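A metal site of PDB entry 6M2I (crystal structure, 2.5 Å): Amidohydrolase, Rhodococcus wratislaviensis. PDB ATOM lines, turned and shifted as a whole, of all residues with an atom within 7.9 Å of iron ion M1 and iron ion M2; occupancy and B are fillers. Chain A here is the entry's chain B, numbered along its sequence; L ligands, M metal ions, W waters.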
ATOM      1  N   ALA A  24      -6.608  -8.792  -1.055  1.00  0.00           N
ATOM      2  CA  ALA A  24      -5.559  -9.365  -0.243  1.00  0.00           C
ATOM      3  C   ALA A  24      -4.688 -10.355  -0.999  1.00  0.00           C
ATOM      4  O   ALA A  24      -3.550 -10.591  -0.562  1.00  0.00           O
ATOM      5  CB  ALA A  24      -6.173 -10.040   0.997  1.00  0.00           C
ATOM      6  N   ASP A  25      -5.138 -10.919  -2.115  1.00  0.00           N
ATOM      7  CA  ASP A  25      -4.420 -12.044  -2.732  1.00  0.00           C
ATOM      8  C   ASP A  25      -4.389 -11.855  -4.249  1.00  0.00           C
ATOM      9  O   ASP A  25      -5.410 -12.047  -4.923  1.00  0.00           O
ATOM     10  CB  ASP A  25      -5.053 -13.381  -2.344  1.00  0.00           C
ATOM     11  CG  ASP A  25      -4.292 -14.586  -2.875  1.00  0.00           C
ATOM     12  OD1 ASP A  25      -3.067 -14.510  -3.107  1.00  0.00           O
ATOM     13  OD2 ASP A  25      -4.903 -15.666  -3.062  1.00  0.00           O
ATOM     14  N   ILE A  26      -3.243 -11.442  -4.769  1.00  0.00           N
ATOM     15  CA  ILE A  26      -3.024 -11.281  -6.204  1.00  0.00           C
ATOM     16  C   ILE A  26      -1.713 -11.955  -6.540  1.00  0.00           C
ATOM     17  O   ILE A  26      -0.698 -11.721  -5.865  1.00  0.00           O
ATOM     18  CB  ILE A  26      -2.969  -9.809  -6.633  1.00  0.00           C
ATOM     19  CG1 ILE A  26      -4.265  -9.082  -6.293  1.00  0.00           C
ATOM     20  CG2 ILE A  26      -2.633  -9.699  -8.110  1.00  0.00           C
ATOM     21  CD1 ILE A  26      -4.114  -7.594  -6.374  1.00  0.00           C
ATOM     22  N   HIS A  27      -1.725 -12.784  -7.583  1.00  0.00           N
ATOM     23  CA  HIS A  27      -0.538 -13.565  -7.934  1.00  0.00           C
ATOM     24  C   HIS A  27       0.089 -13.017  -9.192  1.00  0.00           C
ATOM     25  O   HIS A  27      -0.366 -13.337 -10.307  1.00  0.00           O
ATOM     26  CB  HIS A  27      -0.901 -15.034  -8.102  1.00  0.00           C
ATOM     27  CG  HIS A  27      -1.411 -15.649  -6.829  1.00  0.00           C
ATOM     28  ND1 HIS A  27      -0.649 -15.708  -5.684  1.00  0.00           N
ATOM     29  CD2 HIS A  27      -2.629 -16.142  -6.501  1.00  0.00           C
ATOM     30  CE1 HIS A  27      -1.367 -16.251  -4.721  1.00  0.00           C
ATOM     31  NE2 HIS A  27      -2.570 -16.520  -5.184  1.00  0.00           N
ATOM     32  N   GLN A 106       1.372 -11.794  -3.903  1.00  0.00           N
ATOM     33  CA  GLN A 106       1.773 -13.009  -3.191  1.00  0.00           C
ATOM     34  C   GLN A 106       2.397 -13.949  -4.213  1.00  0.00           C
ATOM     35  O   GLN A 106       1.694 -14.757  -4.830  1.00  0.00           O
ATOM     36  CB  GLN A 106       0.584 -13.626  -2.476  1.00  0.00           C
ATOM     37  CG  GLN A 106       0.049 -12.679  -1.425  1.00  0.00           C
ATOM     38  CD  GLN A 106      -0.950 -13.318  -0.509  1.00  0.00           C
ATOM     39  OE1 GLN A 106      -1.057 -14.548  -0.443  1.00  0.00           O
ATOM     40  NE2 GLN A 106      -1.684 -12.491   0.227  1.00  0.00           N
ATOM     41  N   LEU A 108       4.459 -16.938  -4.887  1.00  0.00           N
ATOM     42  CA  LEU A 108       4.986 -18.166  -4.313  1.00  0.00           C
ATOM     43  C   LEU A 108       5.833 -18.984  -5.295  1.00  0.00           C
ATOM     44  O   LEU A 108       6.665 -19.779  -4.855  1.00  0.00           O
ATOM     45  CB  LEU A 108       3.848 -19.043  -3.783  1.00  0.00           C
ATOM     46  CG  LEU A 108       3.228 -18.639  -2.436  1.00  0.00           C
ATOM     47  CD1 LEU A 108       4.275 -18.212  -1.407  1.00  0.00           C
ATOM     48  CD2 LEU A 108       2.196 -17.557  -2.658  1.00  0.00           C
ATOM     49  N   HIS A 211      -0.462 -18.267   3.074  1.00  0.00           N
ATOM     50  CA  HIS A 211      -1.189 -18.710   1.903  1.00  0.00           C
ATOM     51  C   HIS A 211      -1.273 -20.229   1.880  1.00  0.00           C
ATOM     52  O   HIS A 211      -0.320 -20.917   2.228  1.00  0.00           O
ATOM     53  CB  HIS A 211      -0.501 -18.209   0.640  1.00  0.00           C
ATOM     54  CG  HIS A 211      -1.367 -18.266  -0.579  1.00  0.00           C
ATOM     55  ND1 HIS A 211      -1.536 -19.421  -1.319  1.00  0.00           N
ATOM     56  CD2 HIS A 211      -2.082 -17.312  -1.213  1.00  0.00           C
ATOM     57  CE1 HIS A 211      -2.324 -19.174  -2.343  1.00  0.00           C
ATOM     58  NE2 HIS A 211      -2.674 -17.899  -2.309  1.00  0.00           N
ATOM     59  N   LEU A 212      -2.448 -20.731   1.500  1.00  0.00           N
ATOM     60  CA  LEU A 212      -2.634 -22.109   1.096  1.00  0.00           C
ATOM     61  C   LEU A 212      -1.428 -22.585   0.315  1.00  0.00           C
ATOM     62  O   LEU A 212      -0.981 -21.922  -0.629  1.00  0.00           O
ATOM     63  CB  LEU A 212      -3.890 -22.229   0.225  1.00  0.00           C
ATOM     64  CG  LEU A 212      -4.269 -23.533  -0.515  1.00  0.00           C
ATOM     65  CD1 LEU A 212      -5.715 -23.447  -1.009  1.00  0.00           C
ATOM     66  CD2 LEU A 212      -3.376 -23.852  -1.729  1.00  0.00           C
ATOM     67  N   HIS A 233      -8.262 -30.460  -3.016  1.00  0.00           N
ATOM     68  CA  HIS A 233      -8.556 -29.041  -2.933  1.00  0.00           C
ATOM     69  C   HIS A 233      -9.465 -28.709  -1.751  1.00  0.00           C
ATOM     70  O   HIS A 233      -9.300 -27.661  -1.129  1.00  0.00           O
ATOM     71  CB  HIS A 233      -9.146 -28.542  -4.243  1.00  0.00           C
ATOM     72  CG  HIS A 233      -9.144 -27.056  -4.364  1.00  0.00           C
ATOM     73  ND1 HIS A 233      -9.812 -26.389  -5.363  1.00  0.00           N
ATOM     74  CD2 HIS A 233      -8.570 -26.100  -3.597  1.00  0.00           C
ATOM     75  CE1 HIS A 233      -9.657 -25.090  -5.207  1.00  0.00           C
ATOM     76  NE2 HIS A 233      -8.906 -24.877  -4.142  1.00  0.00           N
ATOM     77  N   VAL A 264      -5.058 -17.209   4.229  1.00  0.00           N
ATOM     78  CA  VAL A 264      -5.363 -16.741   2.883  1.00  0.00           C
ATOM     79  C   VAL A 264      -5.689 -17.962   2.033  1.00  0.00           C
ATOM     80  O   VAL A 264      -4.866 -18.878   1.908  1.00  0.00           O
ATOM     81  CB  VAL A 264      -4.187 -15.956   2.285  1.00  0.00           C
ATOM     82  CG1 VAL A 264      -4.398 -15.772   0.800  1.00  0.00           C
ATOM     83  CG2 VAL A 264      -4.043 -14.626   3.007  1.00  0.00           C
ATOM     84  N   GLU A 265      -6.884 -17.948   1.444  1.00  0.00           N
ATOM     85  CA  GLU A 265      -7.333 -18.988   0.531  1.00  0.00           C
ATOM     86  C   GLU A 265      -7.488 -20.316   1.243  1.00  0.00           C
ATOM     87  O   GLU A 265      -7.237 -21.375   0.665  1.00  0.00           O
ATOM     88  CB  GLU A 265      -6.390 -19.106  -0.666  1.00  0.00           C
ATOM     89  CG  GLU A 265      -7.072 -19.554  -1.939  1.00  0.00           C
ATOM     90  CD  GLU A 265      -6.175 -19.357  -3.126  1.00  0.00           C
ATOM     91  OE1 GLU A 265      -5.397 -18.376  -3.109  1.00  0.00           O
ATOM     92  OE2 GLU A 265      -6.223 -20.173  -4.072  1.00  0.00           O
ATOM     93  N   SER A 307      -8.983 -14.162   4.557  1.00  0.00           N
ATOM     94  CA  SER A 307      -9.477 -13.655   3.293  1.00  0.00           C
ATOM     95  C   SER A 307     -10.636 -14.525   2.788  1.00  0.00           C
ATOM     96  O   SER A 307     -10.812 -15.665   3.208  1.00  0.00           O
ATOM     97  CB  SER A 307      -8.343 -13.601   2.261  1.00  0.00           C
ATOM     98  OG  SER A 307      -7.951 -14.898   1.843  1.00  0.00           O
ATOM     99  N   GLN A 309     -11.644 -15.413  -0.618  1.00  0.00           N
ATOM    100  CA  GLN A 309     -11.595 -16.331  -1.740  1.00  0.00           C
ATOM    101  C   GLN A 309     -11.067 -17.693  -1.285  1.00  0.00           C
ATOM    102  O   GLN A 309     -10.153 -17.765  -0.448  1.00  0.00           O
ATOM    103  CB  GLN A 309     -10.713 -15.758  -2.847  1.00  0.00           C
ATOM    104  CG  GLN A 309     -10.893 -16.431  -4.191  1.00  0.00           C
ATOM    105  CD  GLN A 309      -9.954 -17.607  -4.347  1.00  0.00           C
ATOM    106  OE1 GLN A 309      -8.972 -17.709  -3.613  1.00  0.00           O
ATOM    107  NE2 GLN A 309     -10.249 -18.499  -5.317  1.00  0.00           N
ATOM    108  N   PRO A 310     -11.645 -18.804  -1.770  1.00  0.00           N
ATOM    109  CA  PRO A 310     -12.889 -18.874  -2.548  1.00  0.00           C
ATOM    110  C   PRO A 310     -14.078 -18.792  -1.626  1.00  0.00           C
ATOM    111  O   PRO A 310     -14.118 -19.511  -0.638  1.00  0.00           O
ATOM    112  CB  PRO A 310     -12.823 -20.249  -3.234  1.00  0.00           C
ATOM    113  CG  PRO A 310     -11.996 -21.082  -2.278  1.00  0.00           C
ATOM    114  CD  PRO A 310     -11.018 -20.130  -1.602  1.00  0.00           C
ATOM    115  N   ALA A 335     -10.519 -10.801  -1.267  1.00  0.00           N
ATOM    116  CA  ALA A 335      -9.418 -11.127  -2.175  1.00  0.00           C
ATOM    117  C   ALA A 335      -9.987 -11.700  -3.465  1.00  0.00           C
ATOM    118  O   ALA A 335     -11.017 -12.393  -3.469  1.00  0.00           O
ATOM    119  CB  ALA A 335      -8.434 -12.109  -1.539  1.00  0.00           C
ATOM    120  N   THR A 336      -9.296 -11.424  -4.579  1.00  0.00           N
ATOM    121  CA  THR A 336      -9.708 -11.985  -5.857  1.00  0.00           C
ATOM    122  C   THR A 336      -9.036 -13.317  -6.164  1.00  0.00           C
ATOM    123  O   THR A 336      -9.665 -14.184  -6.779  1.00  0.00           O
ATOM    124  CB  THR A 336      -9.369 -11.028  -7.017  1.00  0.00           C
ATOM    125  OG1 THR A 336      -7.949 -10.829  -7.064  1.00  0.00           O
ATOM    126  CG2 THR A 336     -10.093  -9.687  -6.902  1.00  0.00           C
ATOM    127  N   ASP A 337      -7.763 -13.466  -5.766  1.00  0.00           N
ATOM    128  CA  ASP A 337      -6.920 -14.588  -6.205  1.00  0.00           C
ATOM    129  C   ASP A 337      -6.684 -14.530  -7.711  1.00  0.00           C
ATOM    130  O   ASP A 337      -6.460 -15.564  -8.360  1.00  0.00           O
ATOM    131  CB  ASP A 337      -7.515 -15.933  -5.796  1.00  0.00           C
ATOM    132  CG  ASP A 337      -6.478 -17.038  -5.772  1.00  0.00           C
ATOM    133  OD1 ASP A 337      -5.284 -16.714  -5.738  1.00  0.00           O
ATOM    134  OD2 ASP A 337      -6.857 -18.226  -5.790  1.00  0.00           O
ATOM    135  N   TYR A 338      -6.716 -13.336  -8.269  1.00  0.00           N
ATOM    136  CA  TYR A 338      -6.434 -13.150  -9.677  1.00  0.00           C
ATOM    137  C   TYR A 338      -5.002 -13.569  -9.961  1.00  0.00           C
ATOM    138  O   TYR A 338      -4.089 -13.188  -9.224  1.00  0.00           O
ATOM    139  CB  TYR A 338      -6.664 -11.683 -10.074  1.00  0.00           C
ATOM    140  CG  TYR A 338      -6.360 -11.364 -11.523  1.00  0.00           C
ATOM    141  CD1 TYR A 338      -5.065 -11.094 -11.937  1.00  0.00           C
ATOM    142  CD2 TYR A 338      -7.368 -11.356 -12.480  1.00  0.00           C
ATOM    143  CE1 TYR A 338      -4.773 -10.822 -13.271  1.00  0.00           C
ATOM    144  CE2 TYR A 338      -7.093 -11.087 -13.813  1.00  0.00           C
ATOM    145  CZ  TYR A 338      -5.801 -10.817 -14.193  1.00  0.00           C
ATOM    146  OH  TYR A 338      -5.515 -10.539 -15.507  1.00  0.00           O
ATOM    147  N   PRO A 339      -4.751 -14.311 -11.049  1.00  0.00           N
ATOM    148  CA  PRO A 339      -5.701 -14.700 -12.099  1.00  0.00           C
ATOM    149  C   PRO A 339      -6.156 -16.166 -12.099  1.00  0.00           C
ATOM    150  O   PRO A 339      -6.340 -16.722 -13.176  1.00  0.00           O
ATOM    151  CB  PRO A 339      -4.910 -14.397 -13.372  1.00  0.00           C
ATOM    152  CG  PRO A 339      -3.491 -14.758 -12.982  1.00  0.00           C
ATOM    153  CD  PRO A 339      -3.364 -14.570 -11.481  1.00  0.00           C
ATOM    154  N   HIS A 340      -6.354 -16.770 -10.934  1.00  0.00           N
ATOM    155  CA  HIS A 340      -6.700 -18.190 -10.878  1.00  0.00           C
ATOM    156  C   HIS A 340      -8.124 -18.452 -11.363  1.00  0.00           C
ATOM    157  O   HIS A 340      -8.986 -17.562 -11.346  1.00  0.00           O
ATOM    158  CB  HIS A 340      -6.554 -18.714  -9.446  1.00  0.00           C
ATOM    159  CG  HIS A 340      -5.136 -18.790  -8.990  1.00  0.00           C
ATOM    160  ND1 HIS A 340      -4.773 -19.403  -7.814  1.00  0.00           N
ATOM    161  CD2 HIS A 340      -4.002 -18.335  -9.558  1.00  0.00           C
ATOM    162  CE1 HIS A 340      -3.460 -19.318  -7.669  1.00  0.00           C
ATOM    163  NE2 HIS A 340      -2.966 -18.674  -8.715  1.00  0.00           N
ATOM    164  N   PHE A 341      -8.379 -19.713 -11.736  1.00  0.00           N
ATOM    165  CA  PHE A 341      -9.659 -20.085 -12.336  1.00  0.00           C
ATOM    166  C   PHE A 341     -10.820 -19.834 -11.379  1.00  0.00           C
ATOM    167  O   PHE A 341     -11.893 -19.380 -11.800  1.00  0.00           O
ATOM    168  CB  PHE A 341      -9.634 -21.557 -12.790  1.00  0.00           C
ATOM    169  CG  PHE A 341     -10.063 -22.549 -11.734  1.00  0.00           C
ATOM    170  CD1 PHE A 341      -9.123 -23.105 -10.844  1.00  0.00           C
ATOM    171  CD2 PHE A 341     -11.396 -22.963 -11.638  1.00  0.00           C
ATOM    172  CE1 PHE A 341      -9.517 -24.032  -9.864  1.00  0.00           C
ATOM    173  CE2 PHE A 341     -11.797 -23.885 -10.662  1.00  0.00           C
ATOM    174  CZ  PHE A 341     -10.854 -24.426  -9.779  1.00  0.00           C
ATOM    175  N   ASP A 342     -10.628 -20.105 -10.089  1.00  0.00           N
ATOM    176  CA  ASP A 342     -11.670 -19.878  -9.100  1.00  0.00           C
ATOM    177  C   ASP A 342     -11.640 -18.471  -8.528  1.00  0.00           C
ATOM    178  O   ASP A 342     -12.081 -18.255  -7.389  1.00  0.00           O
ATOM    179  CB  ASP A 342     -11.558 -20.911  -7.967  1.00  0.00           C
ATOM    180  CG  ASP A 342     -10.159 -20.949  -7.378  1.00  0.00           C
ATOM    181  OD1 ASP A 342      -9.292 -20.168  -7.832  1.00  0.00           O
ATOM    182  OD2 ASP A 342      -9.939 -21.782  -6.461  1.00  0.00           O
ATOM    183  N   PHE A 343     -11.123 -17.505  -9.292  1.00  0.00           N
ATOM    184  CA  PHE A 343     -11.026 -16.143  -8.791  1.00  0.00           C
ATOM    185  C   PHE A 343     -12.410 -15.559  -8.519  1.00  0.00           C
ATOM    186  O   PHE A 343     -13.403 -15.933  -9.139  1.00  0.00           O
ATOM    187  CB  PHE A 343     -10.242 -15.273  -9.783  1.00  0.00           C
ATOM    188  CG  PHE A 343     -11.112 -14.433 -10.670  1.00  0.00           C
ATOM    189  CD1 PHE A 343     -11.558 -14.930 -11.881  1.00  0.00           C
ATOM    190  CD2 PHE A 343     -11.455 -13.141 -10.305  1.00  0.00           C
ATOM    191  CE1 PHE A 343     -12.350 -14.171 -12.697  1.00  0.00           C
ATOM    192  CE2 PHE A 343     -12.249 -12.369 -11.121  1.00  0.00           C
ATOM    193  CZ  PHE A 343     -12.703 -12.882 -12.315  1.00  0.00           C
HETATM  194  C1  LIG L   1      -5.787 -23.026  -6.106  1.00  0.00           C
HETATM  195  O1  LIG L   1      -4.557 -22.339  -5.894  1.00  0.00           O
HETATM  196  C2  LIG L   1      -6.572 -22.304  -7.201  1.00  0.00           C
HETATM  197  O2  LIG L   1      -7.143 -21.073  -6.731  1.00  0.00           O
HETATM  198 FE    FE M   1      -4.051 -17.378  -4.085  1.00  0.00          FE
HETATM  199 FE    FE M   2      -5.475 -19.730  -5.935  1.00  0.00          FE
HETATM  200  O   HOH W   1      -3.664 -19.608  -4.880  1.00  0.00           O
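Iron ion M2 is bound by ND1 of His 340, OD2 of Asp 337, OE2 of Glu 265, water W1 and O2 of the ligand. Iron ion M2 has five donor atoms within binding distance. Slightly farther from iron ion M2 lies O1 of the ligand (2.8 Å).
Iron ion M1 is bound by the side-chain carboxylate (OE1) of Glu 265 (1.9 Å), a ring nitrogen (NE2) of His 27 (2.0 Å), the side-chain carboxylate (OD1) of Asp 337 (2.2 Å), the side-chain carboxylate (OD2) of Asp 25 (2.2 Å), a ring nitrogen (NE2) of His 211 (2.3 Å) and water W1 (2.4 Å). Iron ion M1 has six donor atoms within binding distance.
The nearest printed residue that does not touch iron ion M1 is His 340 (4.1 Å).
N of Glu 265 lies within hydrogen-bond range of OG of Ser 307, 3.3 Å away. The backbone carbonyl oxygen of Tyr 338 is in hydrogen-bond range of the backbone NH of His 27, 2.9 Å away. A ring nitrogen (ND1) of His 27 sits at hydrogen-bond distance from the backbone carbonyl oxygen (O) of Gln 106, 2.7 Å away. OE1 of Gln 106 lies close to OD1 of Asp 25, at 3.3 Å. OE1 of Gln 309 sits close to OD2 of Asp 337, at 3.1 Å.
Within 4 Å of iron ion M2: Glu 265, Asp 337 and His 340.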
